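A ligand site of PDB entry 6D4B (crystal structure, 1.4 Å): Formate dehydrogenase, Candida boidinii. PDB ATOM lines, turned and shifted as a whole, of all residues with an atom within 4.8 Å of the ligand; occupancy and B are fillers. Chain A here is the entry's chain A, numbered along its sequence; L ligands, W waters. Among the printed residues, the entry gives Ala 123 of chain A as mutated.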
ATOM      1  N   PHE A  69     -35.357   7.568 -14.726  1.00  0.00           N
ATOM      2  CA  PHE A  69     -35.410   9.036 -14.813  1.00  0.00           C
ATOM      3  C   PHE A  69     -36.601   9.599 -14.069  1.00  0.00           C
ATOM      4  O   PHE A  69     -36.618  10.794 -13.766  1.00  0.00           O
ATOM      5  CB  PHE A  69     -35.413   9.460 -16.288  1.00  0.00           C
ATOM      6  CG  PHE A  69     -34.561   8.553 -17.119  1.00  0.00           C
ATOM      7  CD1 PHE A  69     -33.178   8.605 -17.034  1.00  0.00           C
ATOM      8  CD2 PHE A  69     -35.141   7.539 -17.848  1.00  0.00           C
ATOM      9  CE1 PHE A  69     -32.392   7.700 -17.698  1.00  0.00           C
ATOM     10  CE2 PHE A  69     -34.359   6.601 -18.530  1.00  0.00           C
ATOM     11  CZ  PHE A  69     -32.999   6.691 -18.457  1.00  0.00           C
ATOM     12  N   VAL A  93     -31.368   1.432 -17.114  1.00  0.00           N
ATOM     13  CA  VAL A  93     -30.358   0.650 -16.426  1.00  0.00           C
ATOM     14  C   VAL A  93     -30.292   1.143 -14.988  1.00  0.00           C
ATOM     15  O   VAL A  93     -30.222   2.349 -14.739  1.00  0.00           O
ATOM     16  CB  VAL A  93     -29.002   0.817 -17.121  1.00  0.00           C
ATOM     17  CG1 VAL A  93     -27.868   0.197 -16.298  1.00  0.00           C
ATOM     18  CG2 VAL A  93     -29.038   0.190 -18.509  1.00  0.00           C
ATOM     19  N   GLY A  94     -30.284   0.215 -14.050  1.00  0.00           N
ATOM     20  CA  GLY A  94     -30.191   0.536 -12.638  1.00  0.00           C
ATOM     21  C   GLY A  94     -31.488   0.224 -11.920  1.00  0.00           C
ATOM     22  O   GLY A  94     -32.500   0.854 -12.189  1.00  0.00           O
ATOM     23  N   ASP A  96     -31.963   0.051  -8.410  1.00  0.00           N
ATOM     24  CA  ASP A  96     -31.888   0.422  -6.989  1.00  0.00           C
ATOM     25  C   ASP A  96     -33.135   1.112  -6.459  1.00  0.00           C
ATOM     26  O   ASP A  96     -33.275   1.258  -5.243  1.00  0.00           O
ATOM     27  CB  ASP A  96     -30.740   1.402  -6.824  1.00  0.00           C
ATOM     28  CG  ASP A  96     -30.789   2.477  -7.870  1.00  0.00           C
ATOM     29  OD1 ASP A  96     -30.289   2.205  -8.984  1.00  0.00           O
ATOM     30  OD2 ASP A  96     -31.370   3.551  -7.594  1.00  0.00           O
ATOM     31  N   ASN A 119     -28.074   2.142 -22.616  1.00  0.00           N
ATOM     32  CA  ASN A 119     -27.740   3.569 -22.571  1.00  0.00           C
ATOM     33  C   ASN A 119     -26.396   3.765 -21.890  1.00  0.00           C
ATOM     34  O   ASN A 119     -26.110   4.861 -21.369  1.00  0.00           O
ATOM     35  CB  ASN A 119     -28.838   4.354 -21.892  1.00  0.00           C
ATOM     36  CG  ASN A 119     -29.116   3.852 -20.503  1.00  0.00           C
ATOM     37  OD1 ASN A 119     -28.353   3.058 -19.970  1.00  0.00           O
ATOM     38  ND2 ASN A 119     -30.188   4.329 -19.909  1.00  0.00           N
ATOM     39  N   VAL A 120     -25.539   2.735 -21.906  1.00  0.00           N
ATOM     40  CA  VAL A 120     -24.220   2.841 -21.310  1.00  0.00           C
ATOM     41  C   VAL A 120     -23.326   3.772 -22.113  1.00  0.00           C
ATOM     42  O   VAL A 120     -22.504   4.486 -21.543  1.00  0.00           O
ATOM     43  CB  VAL A 120     -23.596   1.442 -21.113  1.00  0.00           C
ATOM     44  CG1 VAL A 120     -24.502   0.620 -20.206  1.00  0.00           C
ATOM     45  CG2 VAL A 120     -23.357   0.699 -22.433  1.00  0.00           C
ATOM     46  N   ALA A 123     -24.506   7.356 -21.160  1.00  0.00           N
ATOM     47  CA  ALA A 123     -23.960   7.787 -19.875  1.00  0.00           C
ATOM     48  C   ALA A 123     -22.458   8.072 -19.961  1.00  0.00           C
ATOM     49  O   ALA A 123     -21.969   9.057 -19.377  1.00  0.00           O
ATOM     50  CB  ALA A 123     -24.242   6.742 -18.793  1.00  0.00           C
ATOM     51  N   ILE A 170     -14.591   4.664 -10.147  1.00  0.00           N
ATOM     52  CA  ILE A 170     -15.105   3.748  -9.146  1.00  0.00           C
ATOM     53  C   ILE A 170     -16.176   2.943  -9.857  1.00  0.00           C
ATOM     54  O   ILE A 170     -17.284   3.425 -10.139  1.00  0.00           O
ATOM     55  CB  ILE A 170     -15.644   4.510  -7.936  1.00  0.00           C
ATOM     56  CG1 ILE A 170     -14.495   5.219  -7.227  1.00  0.00           C
ATOM     57  CG2 ILE A 170     -16.374   3.573  -6.995  1.00  0.00           C
ATOM     58  CD1 ILE A 170     -14.946   6.332  -6.315  1.00  0.00           C
ATOM     59  N   GLY A 171     -15.829   1.716 -10.195  1.00  0.00           N
ATOM     60  CA  GLY A 171     -16.628   0.885 -11.067  1.00  0.00           C
ATOM     61  C   GLY A 171     -16.074   0.921 -12.469  1.00  0.00           C
ATOM     62  O   GLY A 171     -15.945   1.989 -13.078  1.00  0.00           O
ATOM     63  N   ALA A 172     -15.709  -0.241 -12.983  1.00  0.00           N
ATOM     64  CA  ALA A 172     -15.139  -0.378 -14.305  1.00  0.00           C
ATOM     65  C   ALA A 172     -15.919  -1.421 -15.092  1.00  0.00           C
ATOM     66  O   ALA A 172     -15.363  -2.344 -15.667  1.00  0.00           O
ATOM     67  CB  ALA A 172     -13.643  -0.692 -14.237  1.00  0.00           C
ATOM     68  N   GLY A 173     -17.251  -1.252 -15.109  1.00  0.00           N
ATOM     69  CA  GLY A 173     -18.139  -2.073 -15.915  1.00  0.00           C
ATOM     70  C   GLY A 173     -18.433  -1.435 -17.255  1.00  0.00           C
ATOM     71  O   GLY A 173     -17.552  -0.831 -17.887  1.00  0.00           O
ATOM     72  N   ARG A 174     -19.670  -1.584 -17.728  1.00  0.00           N
ATOM     73  CA  ARG A 174     -19.994  -1.129 -19.067  1.00  0.00           C
ATOM     74  C   ARG A 174     -19.739   0.354 -19.217  1.00  0.00           C
ATOM     75  O   ARG A 174     -19.114   0.788 -20.189  1.00  0.00           O
ATOM     76  CB  ARG A 174     -21.425  -1.512 -19.424  1.00  0.00           C
ATOM     77  CG  ARG A 174     -21.562  -3.019 -19.607  1.00  0.00           C
ATOM     78  CD  ARG A 174     -22.996  -3.430 -19.727  1.00  0.00           C
ATOM     79  NE  ARG A 174     -23.168  -4.884 -19.860  1.00  0.00           N
ATOM     80  CZ  ARG A 174     -23.162  -5.733 -18.837  1.00  0.00           C
ATOM     81  NH1 ARG A 174     -22.976  -5.310 -17.592  1.00  0.00           N
ATOM     82  NH2 ARG A 174     -23.327  -7.033 -19.054  1.00  0.00           N
ATOM     83  N   ILE A 175     -20.220   1.166 -18.272  1.00  0.00           N
ATOM     84  CA  ILE A 175     -20.007   2.609 -18.391  1.00  0.00           C
ATOM     85  C   ILE A 175     -18.581   2.971 -18.040  1.00  0.00           C
ATOM     86  O   ILE A 175     -17.918   3.702 -18.767  1.00  0.00           O
ATOM     87  CB  ILE A 175     -21.021   3.395 -17.544  1.00  0.00           C
ATOM     88  CG1 ILE A 175     -22.431   3.119 -18.058  1.00  0.00           C
ATOM     89  CG2 ILE A 175     -20.694   4.892 -17.598  1.00  0.00           C
ATOM     90  CD1 ILE A 175     -23.533   3.606 -17.125  1.00  0.00           C
ATOM     91  N   GLY A 176     -18.090   2.498 -16.904  1.00  0.00           N
ATOM     92  CA  GLY A 176     -16.763   2.891 -16.469  1.00  0.00           C
ATOM     93  C   GLY A 176     -15.710   2.581 -17.521  1.00  0.00           C
ATOM     94  O   GLY A 176     -14.835   3.411 -17.790  1.00  0.00           O
ATOM     95  N   TYR A 194     -11.056   1.254  -9.579  1.00  0.00           N
ATOM     96  CA  TYR A 194     -11.327   0.474  -8.371  1.00  0.00           C
ATOM     97  C   TYR A 194     -12.616  -0.282  -8.622  1.00  0.00           C
ATOM     98  O   TYR A 194     -13.652   0.322  -8.947  1.00  0.00           O
ATOM     99  CB  TYR A 194     -11.481   1.413  -7.171  1.00  0.00           C
ATOM    100  CG  TYR A 194     -12.065   0.806  -5.925  1.00  0.00           C
ATOM    101  CD1 TYR A 194     -11.289   0.022  -5.093  1.00  0.00           C
ATOM    102  CD2 TYR A 194     -13.377   1.043  -5.563  1.00  0.00           C
ATOM    103  CE1 TYR A 194     -11.802  -0.517  -3.934  1.00  0.00           C
ATOM    104  CE2 TYR A 194     -13.913   0.521  -4.414  1.00  0.00           C
ATOM    105  CZ  TYR A 194     -13.121  -0.273  -3.595  1.00  0.00           C
ATOM    106  OH  TYR A 194     -13.605  -0.829  -2.419  1.00  0.00           O
ATOM    107  N   ASP A 195     -12.569  -1.595  -8.486  1.00  0.00           N
ATOM    108  CA  ASP A 195     -13.724  -2.442  -8.735  1.00  0.00           C
ATOM    109  C   ASP A 195     -13.377  -3.792  -8.145  1.00  0.00           C
ATOM    110  O   ASP A 195     -12.258  -4.244  -8.299  1.00  0.00           O
ATOM    111  CB  ASP A 195     -13.984  -2.543 -10.248  1.00  0.00           C
ATOM    112  CG  ASP A 195     -15.346  -3.110 -10.583  1.00  0.00           C
ATOM    113  OD1 ASP A 195     -15.883  -3.950  -9.818  1.00  0.00           O
ATOM    114  OD2 ASP A 195     -15.907  -2.704 -11.632  1.00  0.00           O
ATOM    115  N   TYR A 196     -14.303  -4.430  -7.413  1.00  0.00           N
ATOM    116  CA  TYR A 196     -14.021  -5.777  -6.955  1.00  0.00           C
ATOM    117  C   TYR A 196     -13.943  -6.767  -8.105  1.00  0.00           C
ATOM    118  O   TYR A 196     -13.396  -7.870  -7.925  1.00  0.00           O
ATOM    119  CB  TYR A 196     -15.032  -6.240  -5.901  1.00  0.00           C
ATOM    120  CG  TYR A 196     -16.511  -6.236  -6.288  1.00  0.00           C
ATOM    121  CD1 TYR A 196     -17.045  -7.227  -7.116  1.00  0.00           C
ATOM    122  CD2 TYR A 196     -17.371  -5.282  -5.797  1.00  0.00           C
ATOM    123  CE1 TYR A 196     -18.399  -7.229  -7.439  1.00  0.00           C
ATOM    124  CE2 TYR A 196     -18.706  -5.262  -6.113  1.00  0.00           C
ATOM    125  CZ  TYR A 196     -19.226  -6.260  -6.926  1.00  0.00           C
ATOM    126  OH  TYR A 196     -20.571  -6.217  -7.209  1.00  0.00           O
ATOM    127  N   GLN A 197     -14.460  -6.400  -9.283  1.00  0.00           N
ATOM    128  CA  GLN A 197     -14.351  -7.192 -10.492  1.00  0.00           C
ATOM    129  C   GLN A 197     -13.217  -6.619 -11.321  1.00  0.00           C
ATOM    130  O   GLN A 197     -13.293  -5.470 -11.785  1.00  0.00           O
ATOM    131  CB  GLN A 197     -15.659  -7.126 -11.302  1.00  0.00           C
ATOM    132  CG  GLN A 197     -15.599  -7.834 -12.656  1.00  0.00           C
ATOM    133  CD  GLN A 197     -15.207  -9.287 -12.553  1.00  0.00           C
ATOM    134  OE1 GLN A 197     -15.818 -10.064 -11.811  1.00  0.00           O
ATOM    135  NE2 GLN A 197     -14.151  -9.675 -13.256  1.00  0.00           N
ATOM    136  N   ASN A 228     -19.084   5.052 -11.331  1.00  0.00           N
ATOM    137  CA  ASN A 228     -19.771   4.227 -12.318  1.00  0.00           C
ATOM    138  C   ASN A 228     -20.081   2.848 -11.768  1.00  0.00           C
ATOM    139  O   ASN A 228     -19.855   1.826 -12.410  1.00  0.00           O
ATOM    140  CB  ASN A 228     -18.937   4.143 -13.587  1.00  0.00           C
ATOM    141  CG  ASN A 228     -18.750   5.496 -14.212  1.00  0.00           C
ATOM    142  OD1 ASN A 228     -19.718   6.066 -14.729  1.00  0.00           O
ATOM    143  ND2 ASN A 228     -17.547   6.070 -14.127  1.00  0.00           N
ATOM    144  N   ALA A 229     -20.582   2.797 -10.561  1.00  0.00           N
ATOM    145  CA  ALA A 229     -21.046   1.554  -9.962  1.00  0.00           C
ATOM    146  C   ALA A 229     -22.530   1.662  -9.669  1.00  0.00           C
ATOM    147  O   ALA A 229     -23.064   2.766  -9.535  1.00  0.00           O
ATOM    148  CB  ALA A 229     -20.287   1.287  -8.651  1.00  0.00           C
ATOM    149  N   PRO A 230     -23.248   0.536  -9.563  1.00  0.00           N
ATOM    150  CA  PRO A 230     -24.660   0.584  -9.204  1.00  0.00           C
ATOM    151  C   PRO A 230     -24.802   0.993  -7.755  1.00  0.00           C
ATOM    152  O   PRO A 230     -23.851   0.952  -6.967  1.00  0.00           O
ATOM    153  CB  PRO A 230     -25.154  -0.870  -9.426  1.00  0.00           C
ATOM    154  CG  PRO A 230     -24.018  -1.549 -10.183  1.00  0.00           C
ATOM    155  CD  PRO A 230     -22.778  -0.846  -9.717  1.00  0.00           C
ATOM    156  N   LEU A 231     -26.001   1.428  -7.405  1.00  0.00           N
ATOM    157  CA  LEU A 231     -26.343   1.716  -6.028  1.00  0.00           C
ATOM    158  C   LEU A 231     -26.836   0.436  -5.370  1.00  0.00           C
ATOM    159  O   LEU A 231     -27.798  -0.176  -5.829  1.00  0.00           O
ATOM    160  CB  LEU A 231     -27.412   2.799  -5.951  1.00  0.00           C
ATOM    161  CG  LEU A 231     -27.991   3.102  -4.566  1.00  0.00           C
ATOM    162  CD1 LEU A 231     -26.903   3.609  -3.607  1.00  0.00           C
ATOM    163  CD2 LEU A 231     -29.122   4.091  -4.676  1.00  0.00           C
ATOM    164  N   HIS A 232     -26.118   0.030  -4.327  1.00  0.00           N
ATOM    165  CA  HIS A 232     -26.488  -1.095  -3.505  1.00  0.00           C
ATOM    166  C   HIS A 232     -25.920  -0.845  -2.117  1.00  0.00           C
ATOM    167  O   HIS A 232     -25.319   0.189  -1.844  1.00  0.00           O
ATOM    168  CB  HIS A 232     -26.014  -2.401  -4.135  1.00  0.00           C
ATOM    169  CG  HIS A 232     -24.530  -2.506  -4.294  1.00  0.00           C
ATOM    170  ND1 HIS A 232     -23.718  -3.002  -3.308  1.00  0.00           N
ATOM    171  CD2 HIS A 232     -23.716  -2.176  -5.324  1.00  0.00           C
ATOM    172  CE1 HIS A 232     -22.463  -2.996  -3.723  1.00  0.00           C
ATOM    173  NE2 HIS A 232     -22.433  -2.506  -4.954  1.00  0.00           N
ATOM    174  N   GLY A 234     -23.394  -1.681  -0.538  1.00  0.00           N
ATOM    175  CA  GLY A 234     -21.969  -1.406  -0.470  1.00  0.00           C
ATOM    176  C   GLY A 234     -21.540  -0.074  -1.066  1.00  0.00           C
ATOM    177  O   GLY A 234     -20.406   0.368  -0.831  1.00  0.00           O
ATOM    178  N   THR A 235     -22.422   0.558  -1.833  1.00  0.00           N
ATOM    179  CA  THR A 235     -22.114   1.865  -2.397  1.00  0.00           C
ATOM    180  C   THR A 235     -23.002   2.974  -1.850  1.00  0.00           C
ATOM    181  O   THR A 235     -22.700   4.150  -2.089  1.00  0.00           O
ATOM    182  CB  THR A 235     -22.218   1.864  -3.931  1.00  0.00           C
ATOM    183  OG1 THR A 235     -23.523   1.435  -4.327  1.00  0.00           O
ATOM    184  CG2 THR A 235     -21.144   0.983  -4.546  1.00  0.00           C
ATOM    185  N   THR A 256     -22.610  10.147 -12.713  1.00  0.00           N
ATOM    186  CA  THR A 256     -23.765   9.772 -13.510  1.00  0.00           C
ATOM    187  C   THR A 256     -24.326   8.424 -13.091  1.00  0.00           C
ATOM    188  O   THR A 256     -25.112   7.817 -13.833  1.00  0.00           O
ATOM    189  CB  THR A 256     -23.384   9.708 -14.984  1.00  0.00           C
ATOM    190  OG1 THR A 256     -22.335   8.766 -15.161  1.00  0.00           O
ATOM    191  CG2 THR A 256     -22.931  11.057 -15.522  1.00  0.00           C
ATOM    192  N   ALA A 257     -23.903   7.897 -11.939  1.00  0.00           N
ATOM    193  CA  ALA A 257     -24.308   6.560 -11.527  1.00  0.00           C
ATOM    194  C   ALA A 257     -25.621   6.642 -10.774  1.00  0.00           C
ATOM    195  O   ALA A 257     -26.689   6.502 -11.375  1.00  0.00           O
ATOM    196  CB  ALA A 257     -23.223   5.908 -10.683  1.00  0.00           C
ATOM    197  N   ARG A 258     -25.549   6.941  -9.475  1.00  0.00           N
ATOM    198  CA  ARG A 258     -26.742   7.197  -8.682  1.00  0.00           C
ATOM    199  C   ARG A 258     -26.415   8.254  -7.636  1.00  0.00           C
ATOM    200  O   ARG A 258     -25.328   8.252  -7.058  1.00  0.00           O
ATOM    201  CB  ARG A 258     -27.256   5.917  -8.003  1.00  0.00           C
ATOM    202  CG  ARG A 258     -27.913   4.945  -8.968  1.00  0.00           C
ATOM    203  CD  ARG A 258     -29.171   5.558  -9.569  1.00  0.00           C
ATOM    204  NE  ARG A 258     -29.936   4.623 -10.386  1.00  0.00           N
ATOM    205  CZ  ARG A 258     -29.994   4.625 -11.705  1.00  0.00           C
ATOM    206  NH1 ARG A 258     -29.253   5.453 -12.422  1.00  0.00           N
ATOM    207  NH2 ARG A 258     -30.788   3.748 -12.316  1.00  0.00           N
ATOM    208  N   ASP A 282     -25.949  13.832 -13.501  1.00  0.00           N
ATOM    209  CA  ASP A 282     -27.362  13.949 -13.802  1.00  0.00           C
ATOM    210  C   ASP A 282     -28.248  13.260 -12.786  1.00  0.00           C
ATOM    211  O   ASP A 282     -29.465  13.369 -12.883  1.00  0.00           O
ATOM    212  CB  ASP A 282     -27.647  13.432 -15.229  1.00  0.00           C
ATOM    213  CG  ASP A 282     -27.260  11.977 -15.459  1.00  0.00           C
ATOM    214  OD1 ASP A 282     -26.310  11.468 -14.813  1.00  0.00           O
ATOM    215  OD2 ASP A 282     -27.925  11.338 -16.305  1.00  0.00           O
ATOM    216  N   VAL A 283     -27.681  12.598 -11.784  1.00  0.00           N
ATOM    217  CA  VAL A 283     -28.440  11.723 -10.907  1.00  0.00           C
ATOM    218  C   VAL A 283     -28.507  12.295  -9.498  1.00  0.00           C
ATOM    219  O   VAL A 283     -27.545  12.873  -8.979  1.00  0.00           O
ATOM    220  CB  VAL A 283     -27.881  10.282 -10.902  1.00  0.00           C
ATOM    221  CG1 VAL A 283     -28.145   9.632 -12.258  1.00  0.00           C
ATOM    222  CG2 VAL A 283     -26.370  10.229 -10.523  1.00  0.00           C
ATOM    223  N   HIS A 311     -31.963  14.180 -14.431  1.00  0.00           N
ATOM    224  CA  HIS A 311     -31.562  12.831 -14.827  1.00  0.00           C
ATOM    225  C   HIS A 311     -32.047  12.534 -16.227  1.00  0.00           C
ATOM    226  O   HIS A 311     -33.176  12.095 -16.441  1.00  0.00           O
ATOM    227  CB  HIS A 311     -32.094  11.799 -13.859  1.00  0.00           C
ATOM    228  CG  HIS A 311     -31.604  10.426 -14.141  1.00  0.00           C
ATOM    229  ND1 HIS A 311     -32.122   9.322 -13.514  1.00  0.00           N
ATOM    230  CD2 HIS A 311     -30.657   9.976 -15.008  1.00  0.00           C
ATOM    231  CE1 HIS A 311     -31.524   8.242 -13.981  1.00  0.00           C
ATOM    232  NE2 HIS A 311     -30.628   8.611 -14.875  1.00  0.00           N
ATOM    233  N   SER A 313     -29.240  11.652 -18.951  1.00  0.00           N
ATOM    234  CA  SER A 313     -28.191  11.204 -19.870  1.00  0.00           C
ATOM    235  C   SER A 313     -28.568   9.888 -20.518  1.00  0.00           C
ATOM    236  O   SER A 313     -28.282   9.675 -21.705  1.00  0.00           O
ATOM    237  CB  SER A 313     -26.833  11.110 -19.182  1.00  0.00           C
ATOM    238  OG  SER A 313     -26.676   9.961 -18.344  1.00  0.00           O
ATOM    239  N   GLY A 314     -29.200   9.010 -19.768  1.00  0.00           N
ATOM    240  CA  GLY A 314     -29.630   7.726 -20.265  1.00  0.00           C
ATOM    241  C   GLY A 314     -30.922   7.738 -21.013  1.00  0.00           C
ATOM    242  O   GLY A 314     -31.415   6.663 -21.376  1.00  0.00           O
ATOM    243  N   ALA A 357     -22.995  -7.560  -9.965  1.00  0.00           N
ATOM    244  CA  ALA A 357     -22.583  -6.155  -9.892  1.00  0.00           C
ATOM    245  C   ALA A 357     -23.212  -5.384  -8.738  1.00  0.00           C
ATOM    246  O   ALA A 357     -22.889  -4.206  -8.536  1.00  0.00           O
ATOM    247  CB  ALA A 357     -22.925  -5.458 -11.212  1.00  0.00           C
ATOM    248  N   TYR A 358     -24.113  -5.998  -7.978  1.00  0.00           N
ATOM    249  CA  TYR A 358     -24.797  -5.335  -6.867  1.00  0.00           C
ATOM    250  C   TYR A 358     -24.255  -5.847  -5.539  1.00  0.00           C
ATOM    251  O   TYR A 358     -25.008  -6.081  -4.592  1.00  0.00           O
ATOM    252  CB  TYR A 358     -26.311  -5.511  -6.991  1.00  0.00           C
ATOM    253  CG  TYR A 358     -26.936  -4.559  -7.972  1.00  0.00           C
ATOM    254  CD1 TYR A 358     -26.686  -4.661  -9.335  1.00  0.00           C
ATOM    255  CD2 TYR A 358     -27.776  -3.548  -7.534  1.00  0.00           C
ATOM    256  CE1 TYR A 358     -27.255  -3.767 -10.223  1.00  0.00           C
ATOM    257  CE2 TYR A 358     -28.332  -2.660  -8.392  1.00  0.00           C
ATOM    258  CZ  TYR A 358     -28.075  -2.760  -9.734  1.00  0.00           C
ATOM    259  OH  TYR A 358     -28.620  -1.840 -10.580  1.00  0.00           O
HETATM  260  P1  LIG L   1     -22.212  -2.659 -14.911  1.00  0.00           P
HETATM  261  O1  LIG L   1     -22.964  -3.699 -14.083  1.00  0.00           O
HETATM  262  O2  LIG L   1     -21.747  -3.087 -16.255  1.00  0.00           O
HETATM  263  O3  LIG L   1     -20.914  -2.175 -14.138  1.00  0.00           O
HETATM  264  C1  LIG L   1     -20.985  -1.828 -12.758  1.00  0.00           C
HETATM  265  C2  LIG L   1     -19.599  -2.076 -12.126  1.00  0.00           C
HETATM  266  O4  LIG L   1     -19.666  -1.581 -10.895  1.00  0.00           O
HETATM  267  C3  LIG L   1     -19.269  -3.546 -12.046  1.00  0.00           C
HETATM  268  O5  LIG L   1     -18.059  -3.864 -12.655  1.00  0.00           O
HETATM  269  C4  LIG L   1     -19.269  -3.701 -10.489  1.00  0.00           C
HETATM  270  O6  LIG L   1     -18.390  -4.821 -10.090  1.00  0.00           O
HETATM  271  C5  LIG L   1     -18.836  -2.539 -10.016  1.00  0.00           C
HETATM  272  N1  LIG L   1     -19.136  -2.285  -8.605  1.00  0.00           N
HETATM  273  C6  LIG L   1     -20.159  -2.693  -7.820  1.00  0.00           C
HETATM  274  N2  LIG L   1     -19.925  -2.247  -6.568  1.00  0.00           N
HETATM  275  C7  LIG L   1     -18.768  -1.564  -6.567  1.00  0.00           C
HETATM  276  C8  LIG L   1     -18.087  -0.958  -5.553  1.00  0.00           C
HETATM  277  N3  LIG L   1     -18.470  -0.859  -4.232  1.00  0.00           N
HETATM  278  N4  LIG L   1     -16.963  -0.324  -5.827  1.00  0.00           N
HETATM  279  C9  LIG L   1     -16.433  -0.337  -7.091  1.00  0.00           C
HETATM  280  N5  LIG L   1     -17.105  -0.971  -8.094  1.00  0.00           N
HETATM  281  C10 LIG L   1     -18.273  -1.589  -7.824  1.00  0.00           C
HETATM  282  O7  LIG L   1     -23.152  -1.392 -14.993  1.00  0.00           O
HETATM  283  P2  LIG L   1     -23.110  -0.078 -15.928  1.00  0.00           P
HETATM  284  O8  LIG L   1     -21.694   0.332 -16.023  1.00  0.00           O
HETATM  285  O9  LIG L   1     -23.867  -0.350 -17.196  1.00  0.00           O
HETATM  286  O10 LIG L   1     -23.956   0.933 -15.063  1.00  0.00           O
HETATM  287  C11 LIG L   1     -23.501   1.338 -13.774  1.00  0.00           C
HETATM  288  C12 LIG L   1     -24.589   2.166 -13.070  1.00  0.00           C
HETATM  289  O11 LIG L   1     -24.677   3.326 -13.728  1.00  0.00           O
HETATM  290  C13 LIG L   1     -25.990   1.505 -13.193  1.00  0.00           C
HETATM  291  O12 LIG L   1     -26.179   0.546 -12.234  1.00  0.00           O
HETATM  292  C14 LIG L   1     -26.874   2.762 -13.107  1.00  0.00           C
HETATM  293  O13 LIG L   1     -27.133   3.023 -11.651  1.00  0.00           O
HETATM  294  C15 LIG L   1     -26.153   3.813 -13.582  1.00  0.00           C
HETATM  295  N6  LIG L   1     -26.569   4.318 -14.860  1.00  0.00           N
HETATM  296  C16 LIG L   1     -26.985   5.645 -15.003  1.00  0.00           C
HETATM  297  C17 LIG L   1     -27.455   6.099 -16.251  1.00  0.00           C
HETATM  298  C18 LIG L   1     -27.916   7.564 -16.402  1.00  0.00           C
HETATM  299  O14 LIG L   1     -28.796   7.856 -17.145  1.00  0.00           O
HETATM  300  N7  LIG L   1     -27.303   8.540 -15.576  1.00  0.00           N
HETATM  301  C19 LIG L   1     -27.555   5.248 -17.302  1.00  0.00           C
HETATM  302  C20 LIG L   1     -27.160   3.928 -17.168  1.00  0.00           C
HETATM  303  C21 LIG L   1     -26.675   3.464 -15.933  1.00  0.00           C
HETATM  304  O   HOH W   1     -27.536  -1.837 -13.038  1.00  0.00           O
HETATM  305  O   HOH W   2     -22.486   5.949 -14.394  1.00  0.00           O
HETATM  306  O   HOH W   3     -25.837  -1.789 -18.325  1.00  0.00           O
HETATM  307  O   HOH W   4     -27.968   1.055  -9.613  1.00  0.00           O
HETATM  308  O   HOH W   5     -15.067  -2.696  -4.917  1.00  0.00           O
HETATM  309  O   HOH W   6     -22.584  -6.299 -14.807  1.00  0.00           O
HETATM  310  O   HOH W   7     -19.474  -7.323 -11.066  1.00  0.00           O
HETATM  311  O   HOH W   8     -25.668  -3.699 -13.946  1.00  0.00           O
HETATM  312  O   HOH W   9     -19.864  -4.993 -16.803  1.00  0.00           O
HETATM  313  O   HOH W  10     -16.173  -0.447  -1.854  1.00  0.00           O
HETATM  314  O   HOH W  11     -19.232   0.841 -14.867  1.00  0.00           O
HETATM  315  O   HOH W  12     -18.009  -5.627 -14.731  1.00  0.00           O
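An oxygen (O5) of the ligand lies within hydrogen-bond range of the side-chain carboxylate of Asp 195, at 2.7 Å. An oxygen (O8) of the ligand lies within hydrogen-bond range of the backbone NH of Ile 175 (2.8 Å). An oxygen (O2) of the ligand lies within hydrogen-bond range of the backbone NH of Arg 174, at 3.0 Å. NH1 of Arg 174 is in salt-bridge range of O2 of the ligand (2.9 Å). The backbone carbonyl oxygen of Thr 256 sits at hydrogen-bond distance from a nitrogen (N7) of the ligand. The backbone NH (N) of Gly 314 is in hydrogen-bond range of an oxygen (O14) of the ligand (2.9 Å). The side-chain carboxylate of Asp 282 lies within hydrogen-bond range of a nitrogen (N7) of the ligand. NE2 of His 232 sits at hydrogen-bond distance from N2 of the ligand (3.0 Å). A ring nitrogen (NE2) of His 311 lies within hydrogen-bond range of an oxygen (O14) of the ligand (3.0 Å). N7 of the ligand is in hydrogen-bond range of OG of Ser 313, at 3.2 Å. The guanidinium group (NH1) of Arg 258 sits close to an oxygen (O13) of the ligand, 3.3 Å away.
Water W6 lies within hydrogen-bond range of O1 of the ligand (2.7 Å) and NH1 of Arg 174 (3.0 Å). Water W9 bridges O2 of the ligand (2.7 Å) and NH1 of Arg 174 (3.2 Å). Water W11 lies within hydrogen-bond range of O of Asn 228 (2.7 Å), O8 of the ligand (2.8 Å), N of Gly 176 (2.9 Å) and N of Gly 173 (2.9 Å). Water W1 lies within hydrogen-bond range of OH of Tyr 358 and O12 of the ligand. Water W10 lies within hydrogen-bond range of the side-chain hydroxyl of Tyr 194 (2.7 Å) and a nitrogen (N3) of the ligand (3.3 Å). Water W2 lies within hydrogen-bond range of OD1 of Asn 228, OG1 of Thr 256, N of Ala 257 and O11 of the ligand.
The side-chain carboxylate (OD2) of Asp 195 sits at hydrogen-bond distance from the backbone NH (N) of Ala 172 (2.8 Å). The side-chain carboxylate (OD2) of Asp 282 lies within hydrogen-bond range of the side-chain hydroxyl (OG) of Ser 313 (2.8 Å). The side-chain hydroxyl of Thr 235 is in hydrogen-bond range of the backbone NH of His 232 (3.0 Å). OG1 of Thr 235 lies within hydrogen-bond range of O of Pro 230, 2.7 Å away. The guanidinium group (NH2) of Arg 258 sits close to the backbone carbonyl oxygen (O) of Gly 94 (3.4 Å). The guanidinium group of Arg 258 lies within salt-bridge range of the side-chain carboxylate of Asp 96 (2.8 Å). The backbone carbonyl oxygen (O) of Tyr 194 sits at hydrogen-bond distance from the backbone NH (N) of Gly 171, 2.9 Å away. N of Asn 228 sits at hydrogen-bond distance from O of Ile 170, at 2.7 Å.
Residues that only touch the ligand: Asn 119 (3.2 Å), Ala 357 (3.2 Å), Val 120 (3.2 Å), Thr 235 (3.3 Å), Tyr 196 (3.3 Å), Gly 173 (3.3 Å), Pro 230 (3.3 Å), Tyr 194 (3.4 Å), Val 93 (3.5 Å), Ala 257 (3.5 Å), Gly 171 (3.5 Å), Ala 229 (3.6 Å), Val 283 (3.6 Å), Phe 69 (3.6 Å), Asn 228 (3.7 Å), Gln 197 (3.8 Å), Tyr 358 (3.8 Å), Ile 170 (3.9 Å) and Ala 123 (3.9 Å). Hydrophobic or aromatic side chains that line the ligand: Phe 69, Val 93, Val 120, Ala 123, Ile 170, Ile 175, Tyr 194, Tyr 196, Ala 229, Pro 230, His 232, Val 283, His 311 and Ala 357. Of the 35 residues printed, 29 come within 4 Å of the ligand.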
